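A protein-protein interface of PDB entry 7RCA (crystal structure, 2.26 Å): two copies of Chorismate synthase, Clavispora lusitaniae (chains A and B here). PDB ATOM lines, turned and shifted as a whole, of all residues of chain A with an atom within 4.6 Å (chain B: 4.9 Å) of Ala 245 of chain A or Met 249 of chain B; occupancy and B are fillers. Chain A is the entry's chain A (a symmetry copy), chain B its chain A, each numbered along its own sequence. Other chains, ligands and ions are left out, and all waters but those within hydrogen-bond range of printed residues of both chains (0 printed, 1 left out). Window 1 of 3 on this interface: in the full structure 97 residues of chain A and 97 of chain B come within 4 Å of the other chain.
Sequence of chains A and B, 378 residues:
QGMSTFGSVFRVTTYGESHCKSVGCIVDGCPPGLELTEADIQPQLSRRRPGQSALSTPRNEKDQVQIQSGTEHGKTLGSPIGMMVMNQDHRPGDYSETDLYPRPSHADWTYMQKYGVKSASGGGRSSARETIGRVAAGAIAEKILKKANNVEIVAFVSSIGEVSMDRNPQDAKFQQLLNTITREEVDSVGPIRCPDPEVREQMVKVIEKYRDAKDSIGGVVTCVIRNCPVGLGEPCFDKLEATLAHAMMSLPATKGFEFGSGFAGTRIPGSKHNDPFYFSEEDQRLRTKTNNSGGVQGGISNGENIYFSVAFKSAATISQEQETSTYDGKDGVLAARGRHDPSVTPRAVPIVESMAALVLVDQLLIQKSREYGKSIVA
ND1 of His 246 of chain B lies within hydrogen-bond range of O of Ala 242 of chain A (3.1 Å). The backbone carbonyl oxygen (O) of Lys 255 of chain B is in hydrogen-bond range of the backbone NH (N) of Phe 259 of chain A (3.0 Å). The backbone NH (N) of Phe 257 of chain B sits at hydrogen-bond distance from the backbone carbonyl oxygen (O) of Phe 257 of chain A.
The backbone carbonyl oxygen (O) of Met 249 of chain B sits at hydrogen-bond distance from the side-chain hydroxyl (OG1) of Thr 254 of chain B (3.2 Å). The side-chain sulfur of Met 249 of chain B lies within hydrogen-bond range of the backbone NH of Gly 256 of chain B. The backbone carbonyl oxygen (O) of Met 248 of chain B sits at hydrogen-bond distance from the side-chain hydroxyl (OG1) of Thr 254 of chain B (3.2 Å). O of Leu 251 of chain B lies within hydrogen-bond range of OG1 of Thr 254 of chain B (3.0 Å). The side-chain hydroxyl (OG) of Ser 250 of chain B sits at hydrogen-bond distance from the backbone carbonyl oxygen (O) of Ala 247 of chain B (3.1 Å).
Among the printed residues, pairs that only touch across the chains: Glu 241 of chain A with Met 249 of chain B, Ala 242 of chain A with Met 249 of chain B, Ala 242 of chain A with Ser 250 of chain B, Thr 243 of chain A with His 246 of chain B, Ala 245 of chain A with Met 249 of chain B, His 246 of chain A with His 246 of chain B, Met 249 of chain A with Ala 245 of chain B, Phe 257 of chain A with Gly 256 of chain B, Phe 259 of chain A with Met 249 of chain B and Phe 259 of chain A with Thr 254 of chain B.
Of the printed residues of chain B, Glu 241 of chain A touches Met 249. Ala 245 of chain A touches just one residue of chain B: Met 249. Of the printed residues of chain A, Ser 250 of chain B touches Ala 242. The nearest residue of chain B that does not touch Ala 245 of chain A is Ala 245 of chain B (4.3 Å). The nearest printed residue of chain A that does not touch Thr 254 of chain B is Glu 241 of chain A (4.6 Å).
Printed residues of chain B that touch a printed residue of chain A: Ala 245, His 246, Met 249, Ser 250, Thr 254, Lys 255, Gly 256 and Phe 257. Hydrophobic or aromatic side chains of chain B that line the printed part of chain A: Ala 245, His 246 and Met 249. Of the 11 printed residues of chain A, 8 touch a printed residue of chain B. Along chain A the printed residues that touch a printed residue of chain B span positions 241 to 259. Among the printed residues, no Asp or Glu carboxylate lies within 4 Å of a Lys or Arg side-chain nitrogen of the other chain.
Ala 245 of chain A touches Met 249 of chain B, and with the chains exchanged Met 249 of chain A touches Ala 245 of chain B. His 246 of chain B touches its own counterpart, His 246 of chain A. Phe 257 of chain A touches its own counterpart, Phe 257 of chain B.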
ATOM      1  N   GLU A 241     -13.104  -3.290 -25.155  1.00  0.00           N
ATOM      2  CA  GLU A 241     -11.653  -3.155 -25.062  1.00  0.00           C
ATOM      3  C   GLU A 241     -10.975  -4.464 -24.686  1.00  0.00           C
ATOM      4  O   GLU A 241      -9.776  -4.622 -24.945  1.00  0.00           O
ATOM      5  CB  GLU A 241     -11.283  -2.063 -24.052  1.00  0.00           C
ATOM      6  CG  GLU A 241     -11.343  -2.498 -22.595  1.00  0.00           C
ATOM      7  CD  GLU A 241     -12.710  -2.259 -21.979  1.00  0.00           C
ATOM      8  OE1 GLU A 241     -13.718  -2.451 -22.689  1.00  0.00           O
ATOM      9  OE2 GLU A 241     -12.776  -1.887 -20.785  1.00  0.00           O
ATOM     10  N   ALA A 242     -11.709  -5.402 -24.090  1.00  0.00           N
ATOM     11  CA  ALA A 242     -11.143  -6.711 -23.789  1.00  0.00           C
ATOM     12  C   ALA A 242     -11.093  -7.593 -25.032  1.00  0.00           C
ATOM     13  O   ALA A 242     -10.098  -8.290 -25.260  1.00  0.00           O
ATOM     14  CB  ALA A 242     -11.949  -7.390 -22.681  1.00  0.00           C
ATOM     15  N   THR A 243     -12.152  -7.575 -25.846  1.00  0.00           N
ATOM     16  CA  THR A 243     -12.120  -8.321 -27.100  1.00  0.00           C
ATOM     17  C   THR A 243     -11.103  -7.734 -28.067  1.00  0.00           C
ATOM     18  O   THR A 243     -10.465  -8.477 -28.820  1.00  0.00           O
ATOM     19  CB  THR A 243     -13.504  -8.338 -27.745  1.00  0.00           C
ATOM     20  OG1 THR A 243     -14.079  -7.027 -27.671  1.00  0.00           O
ATOM     21  CG2 THR A 243     -14.413  -9.331 -27.030  1.00  0.00           C
ATOM     22  N   LEU A 244     -10.937  -6.409 -28.059  1.00  0.00           N
ATOM     23  CA  LEU A 244      -9.935  -5.781 -28.912  1.00  0.00           C
ATOM     24  C   LEU A 244      -8.526  -6.150 -28.468  1.00  0.00           C
ATOM     25  O   LEU A 244      -7.667  -6.449 -29.304  1.00  0.00           O
ATOM     26  CB  LEU A 244     -10.119  -4.265 -28.909  1.00  0.00           C
ATOM     27  CG  LEU A 244     -11.248  -3.726 -29.788  1.00  0.00           C
ATOM     28  CD1 LEU A 244     -11.393  -2.224 -29.604  1.00  0.00           C
ATOM     29  CD2 LEU A 244     -10.999  -4.073 -31.250  1.00  0.00           C
ATOM     30  N   ALA A 245      -8.266  -6.126 -27.160  1.00  0.00           N
ATOM     31  CA  ALA A 245      -6.968  -6.565 -26.662  1.00  0.00           C
ATOM     32  C   ALA A 245      -6.722  -8.029 -26.999  1.00  0.00           C
ATOM     33  O   ALA A 245      -5.624  -8.401 -27.427  1.00  0.00           O
ATOM     34  CB  ALA A 245      -6.880  -6.345 -25.153  1.00  0.00           C
ATOM     35  N   HIS A 246      -7.734  -8.875 -26.796  1.00  0.00           N
ATOM     36  CA  HIS A 246      -7.628 -10.275 -27.189  1.00  0.00           C
ATOM     37  C   HIS A 246      -7.287 -10.398 -28.666  1.00  0.00           C
ATOM     38  O   HIS A 246      -6.416 -11.188 -29.050  1.00  0.00           O
ATOM     39  CB  HIS A 246      -8.938 -10.998 -26.874  1.00  0.00           C
ATOM     40  CG  HIS A 246      -8.925 -12.459 -27.203  1.00  0.00           C
ATOM     41  ND1 HIS A 246      -8.086 -13.356 -26.578  1.00  0.00           N
ATOM     42  CD2 HIS A 246      -9.670 -13.184 -28.070  1.00  0.00           C
ATOM     43  CE1 HIS A 246      -8.304 -14.568 -27.056  1.00  0.00           C
ATOM     44  NE2 HIS A 246      -9.260 -14.491 -27.965  1.00  0.00           N
ATOM     45  N   ALA A 247      -7.946  -9.597 -29.505  1.00  0.00           N
ATOM     46  CA  ALA A 247      -7.726  -9.677 -30.943  1.00  0.00           C
ATOM     47  C   ALA A 247      -6.312  -9.249 -31.316  1.00  0.00           C
ATOM     48  O   ALA A 247      -5.663  -9.891 -32.150  1.00  0.00           O
ATOM     49  CB  ALA A 247      -8.756  -8.817 -31.675  1.00  0.00           C
ATOM     50  N   MET A 248      -5.812  -8.173 -30.708  1.00  0.00           N
ATOM     51  CA  MET A 248      -4.510  -7.661 -31.119  1.00  0.00           C
ATOM     52  C   MET A 248      -3.372  -8.474 -30.518  1.00  0.00           C
ATOM     53  O   MET A 248      -2.369  -8.731 -31.193  1.00  0.00           O
ATOM     54  CB  MET A 248      -4.377  -6.188 -30.740  1.00  0.00           C
ATOM     55  CG  MET A 248      -5.503  -5.319 -31.265  1.00  0.00           C
ATOM     56  SD  MET A 248      -5.554  -5.309 -33.065  1.00  0.00           S
ATOM     57  CE  MET A 248      -7.264  -4.855 -33.353  1.00  0.00           C
ATOM     58  N   MET A 249      -3.507  -8.894 -29.259  1.00  0.00           N
ATOM     59  CA  MET A 249      -2.448  -9.665 -28.621  1.00  0.00           C
ATOM     60  C   MET A 249      -2.343 -11.082 -29.168  1.00  0.00           C
ATOM     61  O   MET A 249      -1.358 -11.765 -28.877  1.00  0.00           O
ATOM     62  CB  MET A 249      -2.669  -9.696 -27.109  1.00  0.00           C
ATOM     63  CG  MET A 249      -2.385  -8.364 -26.427  1.00  0.00           C
ATOM     64  SD  MET A 249      -0.747  -7.697 -26.784  1.00  0.00           S
ATOM     65  CE  MET A 249       0.289  -9.077 -26.298  1.00  0.00           C
ATOM     66  N   PHE A 257      -0.686  -3.958 -25.457  1.00  0.00           N
ATOM     67  CA  PHE A 257      -1.879  -3.303 -25.969  1.00  0.00           C
ATOM     68  C   PHE A 257      -2.342  -2.279 -24.946  1.00  0.00           C
ATOM     69  O   PHE A 257      -2.380  -2.565 -23.747  1.00  0.00           O
ATOM     70  CB  PHE A 257      -2.998  -4.316 -26.256  1.00  0.00           C
ATOM     71  CG  PHE A 257      -4.333  -3.687 -26.582  1.00  0.00           C
ATOM     72  CD1 PHE A 257      -5.232  -3.356 -25.575  1.00  0.00           C
ATOM     73  CD2 PHE A 257      -4.693  -3.443 -27.896  1.00  0.00           C
ATOM     74  CE1 PHE A 257      -6.454  -2.782 -25.876  1.00  0.00           C
ATOM     75  CE2 PHE A 257      -5.916  -2.873 -28.203  1.00  0.00           C
ATOM     76  CZ  PHE A 257      -6.798  -2.544 -27.191  1.00  0.00           C
ATOM     77  N   PHE A 259      -5.247   1.330 -24.778  1.00  0.00           N
ATOM     78  CA  PHE A 259      -6.238   2.148 -25.459  1.00  0.00           C
ATOM     79  C   PHE A 259      -6.559   3.370 -24.610  1.00  0.00           C
ATOM     80  O   PHE A 259      -6.348   3.380 -23.395  1.00  0.00           O
ATOM     81  CB  PHE A 259      -7.516   1.355 -25.768  1.00  0.00           C
ATOM     82  CG  PHE A 259      -8.485   1.285 -24.621  1.00  0.00           C
ATOM     83  CD1 PHE A 259      -8.242   0.448 -23.544  1.00  0.00           C
ATOM     84  CD2 PHE A 259      -9.641   2.049 -24.622  1.00  0.00           C
ATOM     85  CE1 PHE A 259      -9.132   0.376 -22.487  1.00  0.00           C
ATOM     86  CE2 PHE A 259     -10.535   1.979 -23.567  1.00  0.00           C
ATOM     87  CZ  PHE A 259     -10.280   1.142 -22.499  1.00  0.00           C
ATOM     88  N   LEU B 244      -4.627 -13.898 -21.637  1.00  0.00           N
ATOM     89  CA  LEU B 244      -4.262 -13.104 -20.470  1.00  0.00           C
ATOM     90  C   LEU B 244      -4.613 -11.636 -20.671  1.00  0.00           C
ATOM     91  O   LEU B 244      -5.138 -10.989 -19.759  1.00  0.00           O
ATOM     92  CB  LEU B 244      -2.772 -13.263 -20.173  1.00  0.00           C
ATOM     93  CG  LEU B 244      -2.365 -14.553 -19.460  1.00  0.00           C
ATOM     94  CD1 LEU B 244      -0.853 -14.633 -19.331  1.00  0.00           C
ATOM     95  CD2 LEU B 244      -3.034 -14.642 -18.094  1.00  0.00           C
ATOM     96  N   ALA B 245      -4.324 -11.090 -21.853  1.00  0.00           N
ATOM     97  CA  ALA B 245      -4.727  -9.719 -22.146  1.00  0.00           C
ATOM     98  C   ALA B 245      -6.241  -9.574 -22.100  1.00  0.00           C
ATOM     99  O   ALA B 245      -6.764  -8.604 -21.540  1.00  0.00           O
ATOM    100  CB  ALA B 245      -4.193  -9.293 -23.513  1.00  0.00           C
ATOM    101  N   HIS B 246      -6.959 -10.526 -22.700  1.00  0.00           N
ATOM    102  CA  HIS B 246      -8.414 -10.528 -22.617  1.00  0.00           C
ATOM    103  C   HIS B 246      -8.873 -10.528 -21.167  1.00  0.00           C
ATOM    104  O   HIS B 246      -9.779  -9.775 -20.791  1.00  0.00           O
ATOM    105  CB  HIS B 246      -8.970 -11.744 -23.360  1.00  0.00           C
ATOM    106  CG  HIS B 246     -10.465 -11.824 -23.371  1.00  0.00           C
ATOM    107  ND1 HIS B 246     -11.257 -10.878 -23.985  1.00  0.00           N
ATOM    108  CD2 HIS B 246     -11.311 -12.752 -22.868  1.00  0.00           C
ATOM    109  CE1 HIS B 246     -12.527 -11.213 -23.848  1.00  0.00           C
ATOM    110  NE2 HIS B 246     -12.588 -12.346 -23.173  1.00  0.00           N
ATOM    111  N   ALA B 247      -8.232 -11.347 -20.332  1.00  0.00           N
ATOM    112  CA  ALA B 247      -8.633 -11.455 -18.935  1.00  0.00           C
ATOM    113  C   ALA B 247      -8.384 -10.156 -18.181  1.00  0.00           C
ATOM    114  O   ALA B 247      -9.229  -9.718 -17.392  1.00  0.00           O
ATOM    115  CB  ALA B 247      -7.888 -12.612 -18.269  1.00  0.00           C
ATOM    116  N   MET B 248      -7.235  -9.518 -18.410  1.00  0.00           N
ATOM    117  CA  MET B 248      -6.906  -8.335 -17.625  1.00  0.00           C
ATOM    118  C   MET B 248      -7.640  -7.101 -18.133  1.00  0.00           C
ATOM    119  O   MET B 248      -8.098  -6.279 -17.333  1.00  0.00           O
ATOM    120  CB  MET B 248      -5.398  -8.101 -17.627  1.00  0.00           C
ATOM    121  CG  MET B 248      -4.593  -9.305 -17.176  1.00  0.00           C
ATOM    122  SD  MET B 248      -4.968  -9.757 -15.474  1.00  0.00           S
ATOM    123  CE  MET B 248      -4.481 -11.482 -15.467  1.00  0.00           C
ATOM    124  N   MET B 249      -7.770  -6.957 -19.453  1.00  0.00           N
ATOM    125  CA  MET B 249      -8.450  -5.792 -20.004  1.00  0.00           C
ATOM    126  C   MET B 249      -9.955  -5.831 -19.779  1.00  0.00           C
ATOM    127  O   MET B 249     -10.620  -4.814 -19.996  1.00  0.00           O
ATOM    128  CB  MET B 249      -8.141  -5.670 -21.496  1.00  0.00           C
ATOM    129  CG  MET B 249      -6.715  -5.224 -21.785  1.00  0.00           C
ATOM    130  SD  MET B 249      -6.243  -3.698 -20.944  1.00  0.00           S
ATOM    131  CE  MET B 249      -7.547  -2.597 -21.492  1.00  0.00           C
ATOM    132  N   SER B 250     -10.505  -6.970 -19.357  1.00  0.00           N
ATOM    133  CA  SER B 250     -11.908  -7.044 -18.969  1.00  0.00           C
ATOM    134  C   SER B 250     -12.145  -6.569 -17.542  1.00  0.00           C
ATOM    135  O   SER B 250     -13.305  -6.445 -17.129  1.00  0.00           O
ATOM    136  CB  SER B 250     -12.422  -8.477 -19.116  1.00  0.00           C
ATOM    137  OG  SER B 250     -12.227  -9.204 -17.916  1.00  0.00           O
ATOM    138  N   LEU B 251     -11.085  -6.319 -16.780  1.00  0.00           N
ATOM    139  CA  LEU B 251     -11.238  -5.822 -15.429  1.00  0.00           C
ATOM    140  C   LEU B 251     -11.692  -4.364 -15.458  1.00  0.00           C
ATOM    141  O   LEU B 251     -11.459  -3.649 -16.436  1.00  0.00           O
ATOM    142  CB  LEU B 251      -9.925  -5.957 -14.662  1.00  0.00           C
ATOM    143  CG  LEU B 251      -9.449  -7.380 -14.353  1.00  0.00           C
ATOM    144  CD1 LEU B 251      -8.078  -7.361 -13.690  1.00  0.00           C
ATOM    145  CD2 LEU B 251     -10.448  -8.088 -13.469  1.00  0.00           C
ATOM    146  N   THR B 254      -9.163  -0.872 -16.284  1.00  0.00           N
ATOM    147  CA  THR B 254      -7.909  -1.194 -16.952  1.00  0.00           C
ATOM    148  C   THR B 254      -7.828  -0.480 -18.294  1.00  0.00           C
ATOM    149  O   THR B 254      -8.798  -0.443 -19.055  1.00  0.00           O
ATOM    150  CB  THR B 254      -7.762  -2.703 -17.149  1.00  0.00           C
ATOM    151  OG1 THR B 254      -8.892  -3.214 -17.871  1.00  0.00           O
ATOM    152  CG2 THR B 254      -7.652  -3.400 -15.808  1.00  0.00           C
ATOM    153  N   LYS B 255      -6.657   0.092 -18.579  1.00  0.00           N
ATOM    154  CA  LYS B 255      -6.444   0.852 -19.801  1.00  0.00           C
ATOM    155  C   LYS B 255      -5.355   0.288 -20.700  1.00  0.00           C
ATOM    156  O   LYS B 255      -5.178   0.796 -21.814  1.00  0.00           O
ATOM    157  CB  LYS B 255      -6.100   2.314 -19.472  1.00  0.00           C
ATOM    158  CG  LYS B 255      -7.302   3.163 -19.083  1.00  0.00           C
ATOM    159  CD  LYS B 255      -8.278   3.302 -20.240  1.00  0.00           C
ATOM    160  CE  LYS B 255      -9.398   4.272 -19.902  1.00  0.00           C
ATOM    161  NZ  LYS B 255     -10.631   3.985 -20.691  1.00  0.00           N
ATOM    162  N   GLY B 256      -4.623  -0.729 -20.264  1.00  0.00           N
ATOM    163  CA  GLY B 256      -3.545  -1.256 -21.075  1.00  0.00           C
ATOM    164  C   GLY B 256      -2.989  -2.535 -20.494  1.00  0.00           C
ATOM    165  O   GLY B 256      -3.152  -2.825 -19.304  1.00  0.00           O
ATOM    166  N   PHE B 257      -2.318  -3.293 -21.357  1.00  0.00           N
ATOM    167  CA  PHE B 257      -1.715  -4.562 -20.980  1.00  0.00           C
ATOM    168  C   PHE B 257      -0.468  -4.771 -21.824  1.00  0.00           C
ATOM    169  O   PHE B 257      -0.487  -4.544 -23.036  1.00  0.00           O
ATOM    170  CB  PHE B 257      -2.694  -5.731 -21.175  1.00  0.00           C
ATOM    171  CG  PHE B 257      -2.069  -7.096 -21.012  1.00  0.00           C
ATOM    172  CD1 PHE B 257      -1.473  -7.743 -22.088  1.00  0.00           C
ATOM    173  CD2 PHE B 257      -2.091  -7.738 -19.785  1.00  0.00           C
ATOM    174  CE1 PHE B 257      -0.903  -8.994 -21.937  1.00  0.00           C
ATOM    175  CE2 PHE B 257      -1.525  -8.991 -19.629  1.00  0.00           C
ATOM    176  CZ  PHE B 257      -0.932  -9.620 -20.707  1.00  0.00           C
